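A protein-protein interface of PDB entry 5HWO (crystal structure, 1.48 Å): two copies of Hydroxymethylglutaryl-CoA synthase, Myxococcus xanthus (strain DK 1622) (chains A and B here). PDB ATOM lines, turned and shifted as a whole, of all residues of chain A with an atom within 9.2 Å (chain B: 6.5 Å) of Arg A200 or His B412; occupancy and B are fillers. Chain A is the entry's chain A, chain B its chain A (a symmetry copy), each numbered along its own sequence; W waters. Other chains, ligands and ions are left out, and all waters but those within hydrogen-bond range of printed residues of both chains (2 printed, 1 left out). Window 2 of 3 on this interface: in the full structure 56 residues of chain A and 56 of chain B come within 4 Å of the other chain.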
ATOM      1  N   GLU A  85      20.627  26.295  19.455  1.00  0.00           N
ATOM      2  CA  GLU A  85      19.593  25.612  18.688  1.00  0.00           C
ATOM      3  C   GLU A  85      20.148  24.346  18.049  1.00  0.00           C
ATOM      4  O   GLU A  85      19.549  23.790  17.115  1.00  0.00           O
ATOM      5  CB  GLU A  85      18.937  26.540  17.656  1.00  0.00           C
ATOM      6  CG  GLU A  85      19.875  27.120  16.650  1.00  0.00           C
ATOM      7  CD  GLU A  85      19.152  27.846  15.571  1.00  0.00           C
ATOM      8  OE1 GLU A  85      19.110  29.092  15.652  1.00  0.00           O
ATOM      9  OE2 GLU A  85      18.629  27.168  14.646  1.00  0.00           O
ATOM     10  N   THR A  86      21.302  23.885  18.548  1.00  0.00           N
ATOM     11  CA  THR A  86      21.959  22.696  18.037  1.00  0.00           C
ATOM     12  C   THR A  86      22.102  21.708  19.206  1.00  0.00           C
ATOM     13  O   THR A  86      23.175  21.128  19.472  1.00  0.00           O
ATOM     14  CB  THR A  86      23.311  23.052  17.394  1.00  0.00           C
ATOM     15  OG1 THR A  86      23.210  24.231  16.573  1.00  0.00           O
ATOM     16  CG2 THR A  86      23.812  21.899  16.540  1.00  0.00           C
ATOM     17  N   GLY A  87      20.999  21.476  19.904  1.00  0.00           N
ATOM     18  CA  GLY A  87      21.037  20.590  21.050  1.00  0.00           C
ATOM     19  C   GLY A  87      21.319  19.162  20.634  1.00  0.00           C
ATOM     20  O   GLY A  87      21.025  18.745  19.514  1.00  0.00           O
ATOM     21  N   ILE A 148      25.982  25.199  15.345  1.00  0.00           N
ATOM     22  CA  ILE A 148      26.466  24.836  14.016  1.00  0.00           C
ATOM     23  C   ILE A 148      25.302  25.033  13.047  1.00  0.00           C
ATOM     24  O   ILE A 148      24.257  24.383  13.181  1.00  0.00           O
ATOM     25  CB  ILE A 148      27.001  23.397  13.959  1.00  0.00           C
ATOM     26  CG1 ILE A 148      28.179  23.219  14.918  1.00  0.00           C
ATOM     27  CG2 ILE A 148      27.442  23.045  12.526  1.00  0.00           C
ATOM     28  CD1 ILE A 148      27.843  22.716  16.307  1.00  0.00           C
ATOM     29  N   ARG A 150      23.511  24.696   9.639  1.00  0.00           N
ATOM     30  CA  ARG A 150      23.504  23.758   8.521  1.00  0.00           C
ATOM     31  C   ARG A 150      22.192  23.892   7.767  1.00  0.00           C
ATOM     32  O   ARG A 150      21.115  23.686   8.337  1.00  0.00           O
ATOM     33  CB  ARG A 150      23.666  22.339   9.060  1.00  0.00           C
ATOM     34  CG  ARG A 150      23.874  21.304   8.023  1.00  0.00           C
ATOM     35  CD  ARG A 150      23.962  19.963   8.711  1.00  0.00           C
ATOM     36  NE  ARG A 150      23.931  18.890   7.748  1.00  0.00           N
ATOM     37  CZ  ARG A 150      24.855  17.936   7.667  1.00  0.00           C
ATOM     38  NH1 ARG A 150      25.890  17.932   8.498  1.00  0.00           N
ATOM     39  NH2 ARG A 150      24.736  16.984   6.749  1.00  0.00           N
ATOM     40  N   TYR A 151      22.285  24.296   6.510  1.00  0.00           N
ATOM     41  CA  TYR A 151      21.145  24.354   5.611  1.00  0.00           C
ATOM     42  C   TYR A 151      21.137  23.229   4.587  1.00  0.00           C
ATOM     43  O   TYR A 151      20.060  22.784   4.176  1.00  0.00           O
ATOM     44  CB  TYR A 151      21.135  25.716   4.906  1.00  0.00           C
ATOM     45  CG  TYR A 151      20.777  26.866   5.821  1.00  0.00           C
ATOM     46  CD1 TYR A 151      19.445  27.143   6.126  1.00  0.00           C
ATOM     47  CD2 TYR A 151      21.753  27.672   6.372  1.00  0.00           C
ATOM     48  CE1 TYR A 151      19.107  28.185   6.952  1.00  0.00           C
ATOM     49  CE2 TYR A 151      21.418  28.721   7.221  1.00  0.00           C
ATOM     50  CZ  TYR A 151      20.092  28.985   7.479  1.00  0.00           C
ATOM     51  OH  TYR A 151      19.752  30.034   8.289  1.00  0.00           O
ATOM     52  N   TYR A 192       6.588  30.882  11.306  1.00  0.00           N
ATOM     53  CA  TYR A 192       7.383  29.830  10.689  1.00  0.00           C
ATOM     54  C   TYR A 192       8.290  30.412   9.608  1.00  0.00           C
ATOM     55  O   TYR A 192       8.154  30.098   8.422  1.00  0.00           O
ATOM     56  CB  TYR A 192       6.479  28.748  10.106  1.00  0.00           C
ATOM     57  CG  TYR A 192       6.184  27.576  11.020  1.00  0.00           C
ATOM     58  CD1 TYR A 192       7.202  26.779  11.496  1.00  0.00           C
ATOM     59  CD2 TYR A 192       4.877  27.247  11.372  1.00  0.00           C
ATOM     60  CE1 TYR A 192       6.932  25.682  12.313  1.00  0.00           C
ATOM     61  CE2 TYR A 192       4.602  26.156  12.190  1.00  0.00           C
ATOM     62  CZ  TYR A 192       5.629  25.376  12.644  1.00  0.00           C
ATOM     63  OH  TYR A 192       5.409  24.269  13.438  1.00  0.00           O
ATOM     64  N   PHE A 194      11.770  30.223   9.966  1.00  0.00           N
ATOM     65  CA  PHE A 194      12.905  29.313   9.997  1.00  0.00           C
ATOM     66  C   PHE A 194      12.670  28.374  11.171  1.00  0.00           C
ATOM     67  O   PHE A 194      12.205  28.808  12.225  1.00  0.00           O
ATOM     68  CB  PHE A 194      14.203  30.127  10.167  1.00  0.00           C
ATOM     69  CG  PHE A 194      15.406  29.346  10.657  1.00  0.00           C
ATOM     70  CD1 PHE A 194      15.505  28.952  11.971  1.00  0.00           C
ATOM     71  CD2 PHE A 194      16.485  29.110   9.824  1.00  0.00           C
ATOM     72  CE1 PHE A 194      16.619  28.277  12.429  1.00  0.00           C
ATOM     73  CE2 PHE A 194      17.602  28.447  10.281  1.00  0.00           C
ATOM     74  CZ  PHE A 194      17.671  28.016  11.574  1.00  0.00           C
ATOM     75  N   TRP A 195      12.973  27.096  10.988  1.00  0.00           N
ATOM     76  CA  TRP A 195      12.786  26.118  12.055  1.00  0.00           C
ATOM     77  C   TRP A 195      13.540  24.847  11.671  1.00  0.00           C
ATOM     78  O   TRP A 195      14.028  24.713  10.559  1.00  0.00           O
ATOM     79  CB  TRP A 195      11.296  25.870  12.360  1.00  0.00           C
ATOM     80  CG  TRP A 195      10.457  25.124  11.323  1.00  0.00           C
ATOM     81  CD1 TRP A 195       9.936  23.865  11.467  1.00  0.00           C
ATOM     82  CD2 TRP A 195       9.984  25.605  10.048  1.00  0.00           C
ATOM     83  NE1 TRP A 195       9.187  23.529  10.356  1.00  0.00           N
ATOM     84  CE2 TRP A 195       9.209  24.575   9.474  1.00  0.00           C
ATOM     85  CE3 TRP A 195      10.141  26.809   9.329  1.00  0.00           C
ATOM     86  CZ2 TRP A 195       8.591  24.707   8.234  1.00  0.00           C
ATOM     87  CZ3 TRP A 195       9.517  26.922   8.087  1.00  0.00           C
ATOM     88  CH2 TRP A 195       8.759  25.871   7.560  1.00  0.00           C
ATOM     89  N   ARG A 196      13.658  23.919  12.617  1.00  0.00           N
ATOM     90  CA  ARG A 196      14.363  22.667  12.347  1.00  0.00           C
ATOM     91  C   ARG A 196      13.769  21.542  13.181  1.00  0.00           C
ATOM     92  O   ARG A 196      14.136  21.348  14.349  1.00  0.00           O
ATOM     93  CB  ARG A 196      15.865  22.812  12.579  1.00  0.00           C
ATOM     94  CG  ARG A 196      16.609  21.574  12.136  1.00  0.00           C
ATOM     95  CD  ARG A 196      18.098  21.784  12.090  1.00  0.00           C
ATOM     96  NE  ARG A 196      18.751  21.968  13.382  1.00  0.00           N
ATOM     97  CZ  ARG A 196      19.282  20.988  14.115  1.00  0.00           C
ATOM     98  NH1 ARG A 196      19.197  19.717  13.740  1.00  0.00           N
ATOM     99  NH2 ARG A 196      19.908  21.284  15.237  1.00  0.00           N
ATOM    100  N   PRO A 197      12.834  20.779  12.613  1.00  0.00           N
ATOM    101  CA  PRO A 197      12.166  19.720  13.375  1.00  0.00           C
ATOM    102  C   PRO A 197      13.155  18.701  13.917  1.00  0.00           C
ATOM    103  O   PRO A 197      14.240  18.493  13.370  1.00  0.00           O
ATOM    104  CB  PRO A 197      11.225  19.094  12.340  1.00  0.00           C
ATOM    105  CG  PRO A 197      10.928  20.179  11.394  1.00  0.00           C
ATOM    106  CD  PRO A 197      12.159  21.032  11.322  1.00  0.00           C
ATOM    107  N   VAL A 198      12.758  18.058  15.014  1.00  0.00           N
ATOM    108  CA  VAL A 198      13.569  16.985  15.583  1.00  0.00           C
ATOM    109  C   VAL A 198      13.734  15.898  14.532  1.00  0.00           C
ATOM    110  O   VAL A 198      12.772  15.512  13.856  1.00  0.00           O
ATOM    111  CB  VAL A 198      12.913  16.453  16.863  1.00  0.00           C
ATOM    112  CG1 VAL A 198      13.691  15.266  17.371  1.00  0.00           C
ATOM    113  CG2 VAL A 198      12.871  17.543  17.897  1.00  0.00           C
ATOM    114  N   GLY A 199      14.956  15.420  14.362  1.00  0.00           N
ATOM    115  CA  GLY A 199      15.207  14.428  13.329  1.00  0.00           C
ATOM    116  C   GLY A 199      15.577  14.985  11.968  1.00  0.00           C
ATOM    117  O   GLY A 199      15.828  14.195  11.041  1.00  0.00           O
ATOM    118  N   ARG A 200      15.622  16.304  11.814  1.00  0.00           N
ATOM    119  CA  ARG A 200      16.147  16.940  10.614  1.00  0.00           C
ATOM    120  C   ARG A 200      17.465  17.605  10.962  1.00  0.00           C
ATOM    121  O   ARG A 200      17.510  18.501  11.812  1.00  0.00           O
ATOM    122  CB  ARG A 200      15.192  17.997  10.060  1.00  0.00           C
ATOM    123  CG  ARG A 200      14.050  17.389   9.314  1.00  0.00           C
ATOM    124  CD  ARG A 200      13.202  18.415   8.588  1.00  0.00           C
ATOM    125  NE  ARG A 200      12.346  17.639   7.692  1.00  0.00           N
ATOM    126  CZ  ARG A 200      12.568  17.476   6.389  1.00  0.00           C
ATOM    127  NH1 ARG A 200      13.566  18.112   5.805  1.00  0.00           N
ATOM    128  NH2 ARG A 200      11.747  16.713   5.673  1.00  0.00           N
ATOM    129  N   ARG A 201      18.509  17.207  10.261  1.00  0.00           N
ATOM    130  CA  ARG A 201      19.820  17.775  10.474  1.00  0.00           C
ATOM    131  C   ARG A 201      19.968  19.160   9.858  1.00  0.00           C
ATOM    132  O   ARG A 201      20.821  19.922  10.302  1.00  0.00           O
ATOM    133  CB  ARG A 201      20.855  16.819   9.896  1.00  0.00           C
ATOM    134  CG  ARG A 201      22.140  16.875  10.589  1.00  0.00           C
ATOM    135  CD  ARG A 201      22.905  15.611  10.374  1.00  0.00           C
ATOM    136  NE  ARG A 201      24.224  15.738  10.953  1.00  0.00           N
ATOM    137  CZ  ARG A 201      25.292  15.128  10.473  1.00  0.00           C
ATOM    138  NH1 ARG A 201      25.185  14.371   9.392  1.00  0.00           N
ATOM    139  NH2 ARG A 201      26.465  15.307  11.055  1.00  0.00           N
ATOM    140  N   GLU A 202      19.171  19.495   8.842  1.00  0.00           N
ATOM    141  CA  GLU A 202      19.257  20.773   8.145  1.00  0.00           C
ATOM    142  C   GLU A 202      18.009  21.602   8.411  1.00  0.00           C
ATOM    143  O   GLU A 202      16.904  21.062   8.511  1.00  0.00           O
ATOM    144  CB  GLU A 202      19.337  20.566   6.631  1.00  0.00           C
ATOM    145  CG  GLU A 202      20.689  20.122   6.117  1.00  0.00           C
ATOM    146  CD  GLU A 202      20.721  18.661   5.726  1.00  0.00           C
ATOM    147  OE1 GLU A 202      21.042  17.847   6.600  1.00  0.00           O
ATOM    148  OE2 GLU A 202      20.425  18.335   4.547  1.00  0.00           O
ATOM    149  N   ALA A 203      18.195  22.920   8.505  1.00  0.00           N
ATOM    150  CA  ALA A 203      17.098  23.833   8.789  1.00  0.00           C
ATOM    151  C   ALA A 203      16.162  23.980   7.589  1.00  0.00           C
ATOM    152  O   ALA A 203      16.552  23.799   6.426  1.00  0.00           O
ATOM    153  CB  ALA A 203      17.653  25.198   9.181  1.00  0.00           C
ATOM    154  N   LEU A 204      14.914  24.312   7.898  1.00  0.00           N
ATOM    155  CA  LEU A 204      13.910  24.722   6.922  1.00  0.00           C
ATOM    156  C   LEU A 204      13.755  26.230   7.037  1.00  0.00           C
ATOM    157  O   LEU A 204      13.789  26.775   8.146  1.00  0.00           O
ATOM    158  CB  LEU A 204      12.571  24.054   7.245  1.00  0.00           C
ATOM    159  CG  LEU A 204      12.602  22.537   7.159  1.00  0.00           C
ATOM    160  CD1 LEU A 204      11.323  21.974   7.761  1.00  0.00           C
ATOM    161  CD2 LEU A 204      12.769  22.096   5.741  1.00  0.00           C
ATOM    162  N   VAL A 205      13.603  26.912   5.900  1.00  0.00           N
ATOM    163  CA  VAL A 205      13.575  28.373   5.934  1.00  0.00           C
ATOM    164  C   VAL A 205      12.820  28.914   4.733  1.00  0.00           C
ATOM    165  O   VAL A 205      12.951  28.418   3.615  1.00  0.00           O
ATOM    166  CB  VAL A 205      15.008  28.957   6.030  1.00  0.00           C
ATOM    167  CG1 VAL A 205      15.852  28.537   4.846  1.00  0.00           C
ATOM    168  CG2 VAL A 205      14.980  30.474   6.171  1.00  0.00           C
ATOM    169  N   ASP B  89      11.117  20.927  18.404  1.00  0.00           N
ATOM    170  CA  ASP B  89      11.899  21.542  17.348  1.00  0.00           C
ATOM    171  C   ASP B  89      13.250  21.894  17.946  1.00  0.00           C
ATOM    172  O   ASP B  89      13.338  22.267  19.118  1.00  0.00           O
ATOM    173  CB  ASP B  89      11.210  22.811  16.807  1.00  0.00           C
ATOM    174  CG  ASP B  89      11.730  23.215  15.425  1.00  0.00           C
ATOM    175  OD1 ASP B  89      11.169  22.717  14.421  1.00  0.00           O
ATOM    176  OD2 ASP B  89      12.689  24.035  15.338  1.00  0.00           O
ATOM    177  N   HIS B  90      14.302  21.808  17.134  1.00  0.00           N
ATOM    178  CA  HIS B  90      15.614  22.209  17.624  1.00  0.00           C
ATOM    179  C   HIS B  90      15.740  23.714  17.791  1.00  0.00           C
ATOM    180  O   HIS B  90      16.586  24.177  18.564  1.00  0.00           O
ATOM    181  CB  HIS B  90      16.692  21.758  16.647  1.00  0.00           C
ATOM    182  CG  HIS B  90      16.964  20.292  16.668  1.00  0.00           C
ATOM    183  ND1 HIS B  90      17.589  19.671  17.723  1.00  0.00           N
ATOM    184  CD2 HIS B  90      16.726  19.331  15.747  1.00  0.00           C
ATOM    185  CE1 HIS B  90      17.723  18.382  17.454  1.00  0.00           C
ATOM    186  NE2 HIS B  90      17.215  18.153  16.256  1.00  0.00           N
ATOM    187  N   ILE B 409       0.698  17.427  10.919  1.00  0.00           N
ATOM    188  CA  ILE B 409       1.883  18.142  10.474  1.00  0.00           C
ATOM    189  C   ILE B 409       1.771  18.208   8.960  1.00  0.00           C
ATOM    190  O   ILE B 409       1.558  17.180   8.312  1.00  0.00           O
ATOM    191  CB  ILE B 409       3.180  17.450  10.933  1.00  0.00           C
ATOM    192  CG1 ILE B 409       3.164  17.306  12.468  1.00  0.00           C
ATOM    193  CG2 ILE B 409       4.370  18.256  10.479  1.00  0.00           C
ATOM    194  CD1 ILE B 409       4.425  16.733  13.089  1.00  0.00           C
ATOM    195  N   ARG B 410       1.844  19.410   8.408  1.00  0.00           N
ATOM    196  CA  ARG B 410       1.656  19.629   6.977  1.00  0.00           C
ATOM    197  C   ARG B 410       2.816  20.489   6.521  1.00  0.00           C
ATOM    198  O   ARG B 410       3.030  21.575   7.068  1.00  0.00           O
ATOM    199  CB  ARG B 410       0.329  20.347   6.688  1.00  0.00           C
ATOM    200  CG  ARG B 410      -0.940  19.506   6.895  1.00  0.00           C
ATOM    201  CD  ARG B 410      -1.283  18.619   5.679  1.00  0.00           C
ATOM    202  NE  ARG B 410      -0.929  19.213   4.387  1.00  0.00           N
ATOM    203  CZ  ARG B 410      -1.784  19.757   3.519  1.00  0.00           C
ATOM    204  NH1 ARG B 410      -3.083  19.819   3.781  1.00  0.00           N
ATOM    205  NH2 ARG B 410      -1.329  20.256   2.376  1.00  0.00           N
ATOM    206  N   ASP B 411       3.564  20.005   5.529  1.00  0.00           N
ATOM    207  CA  ASP B 411       4.712  20.744   5.016  1.00  0.00           C
ATOM    208  C   ASP B 411       5.641  21.151   6.161  1.00  0.00           C
ATOM    209  O   ASP B 411       6.162  22.265   6.209  1.00  0.00           O
ATOM    210  CB  ASP B 411       4.249  21.955   4.202  1.00  0.00           C
ATOM    211  CG  ASP B 411       3.191  21.594   3.177  1.00  0.00           C
ATOM    212  OD1 ASP B 411       3.399  20.616   2.433  1.00  0.00           O
ATOM    213  OD2 ASP B 411       2.143  22.272   3.133  1.00  0.00           O
ATOM    214  N   HIS B 412       5.821  20.233   7.108  1.00  0.00           N
ATOM    215  CA  HIS B 412       6.717  20.357   8.255  1.00  0.00           C
ATOM    216  C   HIS B 412       6.246  21.383   9.275  1.00  0.00           C
ATOM    217  O   HIS B 412       6.981  21.684  10.223  1.00  0.00           O
ATOM    218  CB  HIS B 412       8.171  20.622   7.818  1.00  0.00           C
ATOM    219  CG  HIS B 412       8.641  19.701   6.737  1.00  0.00           C
ATOM    220  ND1 HIS B 412       8.681  20.074   5.412  1.00  0.00           N
ATOM    221  CD2 HIS B 412       9.054  18.413   6.779  1.00  0.00           C
ATOM    222  CE1 HIS B 412       9.122  19.064   4.685  1.00  0.00           C
ATOM    223  NE2 HIS B 412       9.348  18.041   5.489  1.00  0.00           N
ATOM    224  N   ARG B 413       5.027  21.898   9.132  1.00  0.00           N
ATOM    225  CA  ARG B 413       4.455  22.877  10.047  1.00  0.00           C
ATOM    226  C   ARG B 413       3.399  22.185  10.901  1.00  0.00           C
ATOM    227  O   ARG B 413       2.491  21.538  10.372  1.00  0.00           O
ATOM    228  CB  ARG B 413       3.830  24.053   9.285  1.00  0.00           C
ATOM    229  CG  ARG B 413       4.822  24.907   8.507  1.00  0.00           C
ATOM    230  CD  ARG B 413       4.067  25.944   7.648  1.00  0.00           C
ATOM    231  NE  ARG B 413       4.943  26.814   6.866  1.00  0.00           N
ATOM    232  CZ  ARG B 413       5.505  26.485   5.707  1.00  0.00           C
ATOM    233  NH1 ARG B 413       5.311  25.282   5.183  1.00  0.00           N
ATOM    234  NH2 ARG B 413       6.285  27.364   5.081  1.00  0.00           N
ATOM    235  N   ARG B 414       3.518  22.331  12.205  1.00  0.00           N
ATOM    236  CA  ARG B 414       2.572  21.723  13.127  1.00  0.00           C
ATOM    237  C   ARG B 414       1.305  22.555  13.178  1.00  0.00           C
ATOM    238  O   ARG B 414       1.359  23.789  13.293  1.00  0.00           O
ATOM    239  CB  ARG B 414       3.198  21.617  14.515  1.00  0.00           C
ATOM    240  CG  ARG B 414       4.571  20.938  14.472  1.00  0.00           C
ATOM    241  CD  ARG B 414       5.288  20.971  15.806  1.00  0.00           C
ATOM    242  NE  ARG B 414       4.707  20.064  16.792  1.00  0.00           N
ATOM    243  CZ  ARG B 414       5.032  18.780  16.939  1.00  0.00           C
ATOM    244  NH1 ARG B 414       5.950  18.212  16.153  1.00  0.00           N
ATOM    245  NH2 ARG B 414       4.436  18.054  17.888  1.00  0.00           N
ATOM    246  N   GLN B 415       0.168  21.870  13.115  1.00  0.00           N
ATOM    247  CA  GLN B 415      -1.146  22.493  13.136  1.00  0.00           C
ATOM    248  C   GLN B 415      -1.888  22.071  14.394  1.00  0.00           C
ATOM    249  O   GLN B 415      -1.776  20.920  14.845  1.00  0.00           O
ATOM    250  CB  GLN B 415      -1.974  22.062  11.922  1.00  0.00           C
ATOM    251  CG  GLN B 415      -1.225  22.162  10.598  1.00  0.00           C
ATOM    252  CD  GLN B 415      -0.908  23.602  10.234  1.00  0.00           C
ATOM    253  OE1 GLN B 415      -1.755  24.494  10.378  1.00  0.00           O
ATOM    254  NE2 GLN B 415       0.314  23.839   9.762  1.00  0.00           N
HETATM  255  O   HOH W   1       6.464  30.023   6.385  1.00  0.00           O
HETATM  256  O   HOH W   2      18.289  22.478  19.961  1.00  0.00           O
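The guanidinium group (NH2) of Arg A196 lies within hydrogen-bond range of the backbone carbonyl oxygen (O) of Glu A85 (3.2 Å).
NH1 of Arg A196 lies within hydrogen-bond range of O of Arg A200 (2.8 Å).
NE2 of Gln B415 lies within hydrogen-bond range of O of Arg B413.
The backbone carbonyl oxygen of Trp A195 sits at hydrogen-bond distance from the backbone NH of Leu A204 (2.8 Å).
NH1 of Arg B413 lies within hydrogen-bond range of O of Asp B411 (3.3 Å).
NH2 of Arg A200 is in hydrogen-bond range of NE2 of His B412, at 2.7 Å.
The backbone NH of His B90 lies within hydrogen-bond range of the backbone carbonyl oxygen of Arg A196 (2.8 Å).
The backbone nitrogen (N) of Pro A197 lies close to the side-chain carboxylate (OD1) of Asp B89, at 3.1 Å.
The side-chain carboxylate (OD2) of Asp B89 sits at hydrogen-bond distance from the backbone NH (N) of Arg A196 (2.9 Å).
The indole nitrogen (NE1) of Trp A195 is in hydrogen-bond range of the backbone carbonyl oxygen (O) of His B412 (2.9 Å).
O of Glu A85 sits close to O of His B90 (3.3 Å).
The side-chain hydroxyl (OH) of Tyr A192 lies within hydrogen-bond range of the backbone NH (N) of Arg B414 (3.0 Å).
Of the 9 printed residues of chain B, 6 touch a printed residue of chain A.
Of the 19 printed residues of chain A, 9 touch a printed residue of chain B.
Printed residues of chain A that touch a printed residue of chain B: Glu A85, Gly A87, Tyr A192, Trp A195, Arg A196, Pro A197, Val A198, Arg A200 and Leu A204.
Hydrophobic or aromatic side chains of chain A within 4 Å of the printed part of chain B: Tyr A192, Trp A195, Pro A197, Val A198 and Leu A204.
Along chain A the printed residues that touch a printed residue of chain B span positions 85 to 204.
Among the printed residues, 16 pairs touch across the chains.
His B90 touches Gly A87.
Tyr A192 touches Arg B413.
Trp A195 touches Asp B89.
Asp B411 touches Trp A195 (O to CZ2, 3.996 Å).
Arg B413 touches Trp A195.
His B90 touches Pro A197.
Val A198 touches Asp B89.
CA of Val A198 touches NE2 of His B90 (3.9 Å).
Leu A204 touches His B412 (CD1 to CB, 3.4 Å).
No position is printed for both chains.
Of the 16 pairs that touch across the chains among the printed residues, none has its exchanged pair printed and touching as well.
Arg A200 touches just one residue of chain B: His B412 (2.7 Å).
Of the printed residues of chain A, Asp B411 touches Trp A195 (3.996 Å).
Printed residues of chain A within 4 Å of His B90: Glu A85 (3.3 Å), Gly A87 (3.9 Å), Arg A196 (2.8 Å), Pro A197 (3.5 Å) and Val A198 (3.9 Å).
Printed residues of chain B within 4 Å of Arg A196: Asp B89 (2.9 Å) and His B90 (2.8 Å).
Val A205 touches none of the printed residues of chain B.
Thr A86 touches none of the printed residues of chain B.
The nearest printed residue of chain B that does not touch Tyr A192 is His B412 (4.4 Å).
Water W1 lies within hydrogen-bond range of the backbone carbonyl oxygen (O) of Tyr A192 and the guanidinium group (NH2) of Arg B413.
Water W2 lies within hydrogen-bond range of the backbone carbonyl oxygen (O) of His B90 (2.8 Å), the backbone NH (N) of Gly A87 (2.9 Å) and the backbone carbonyl oxygen (O) of Glu A85 (3.4 Å).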
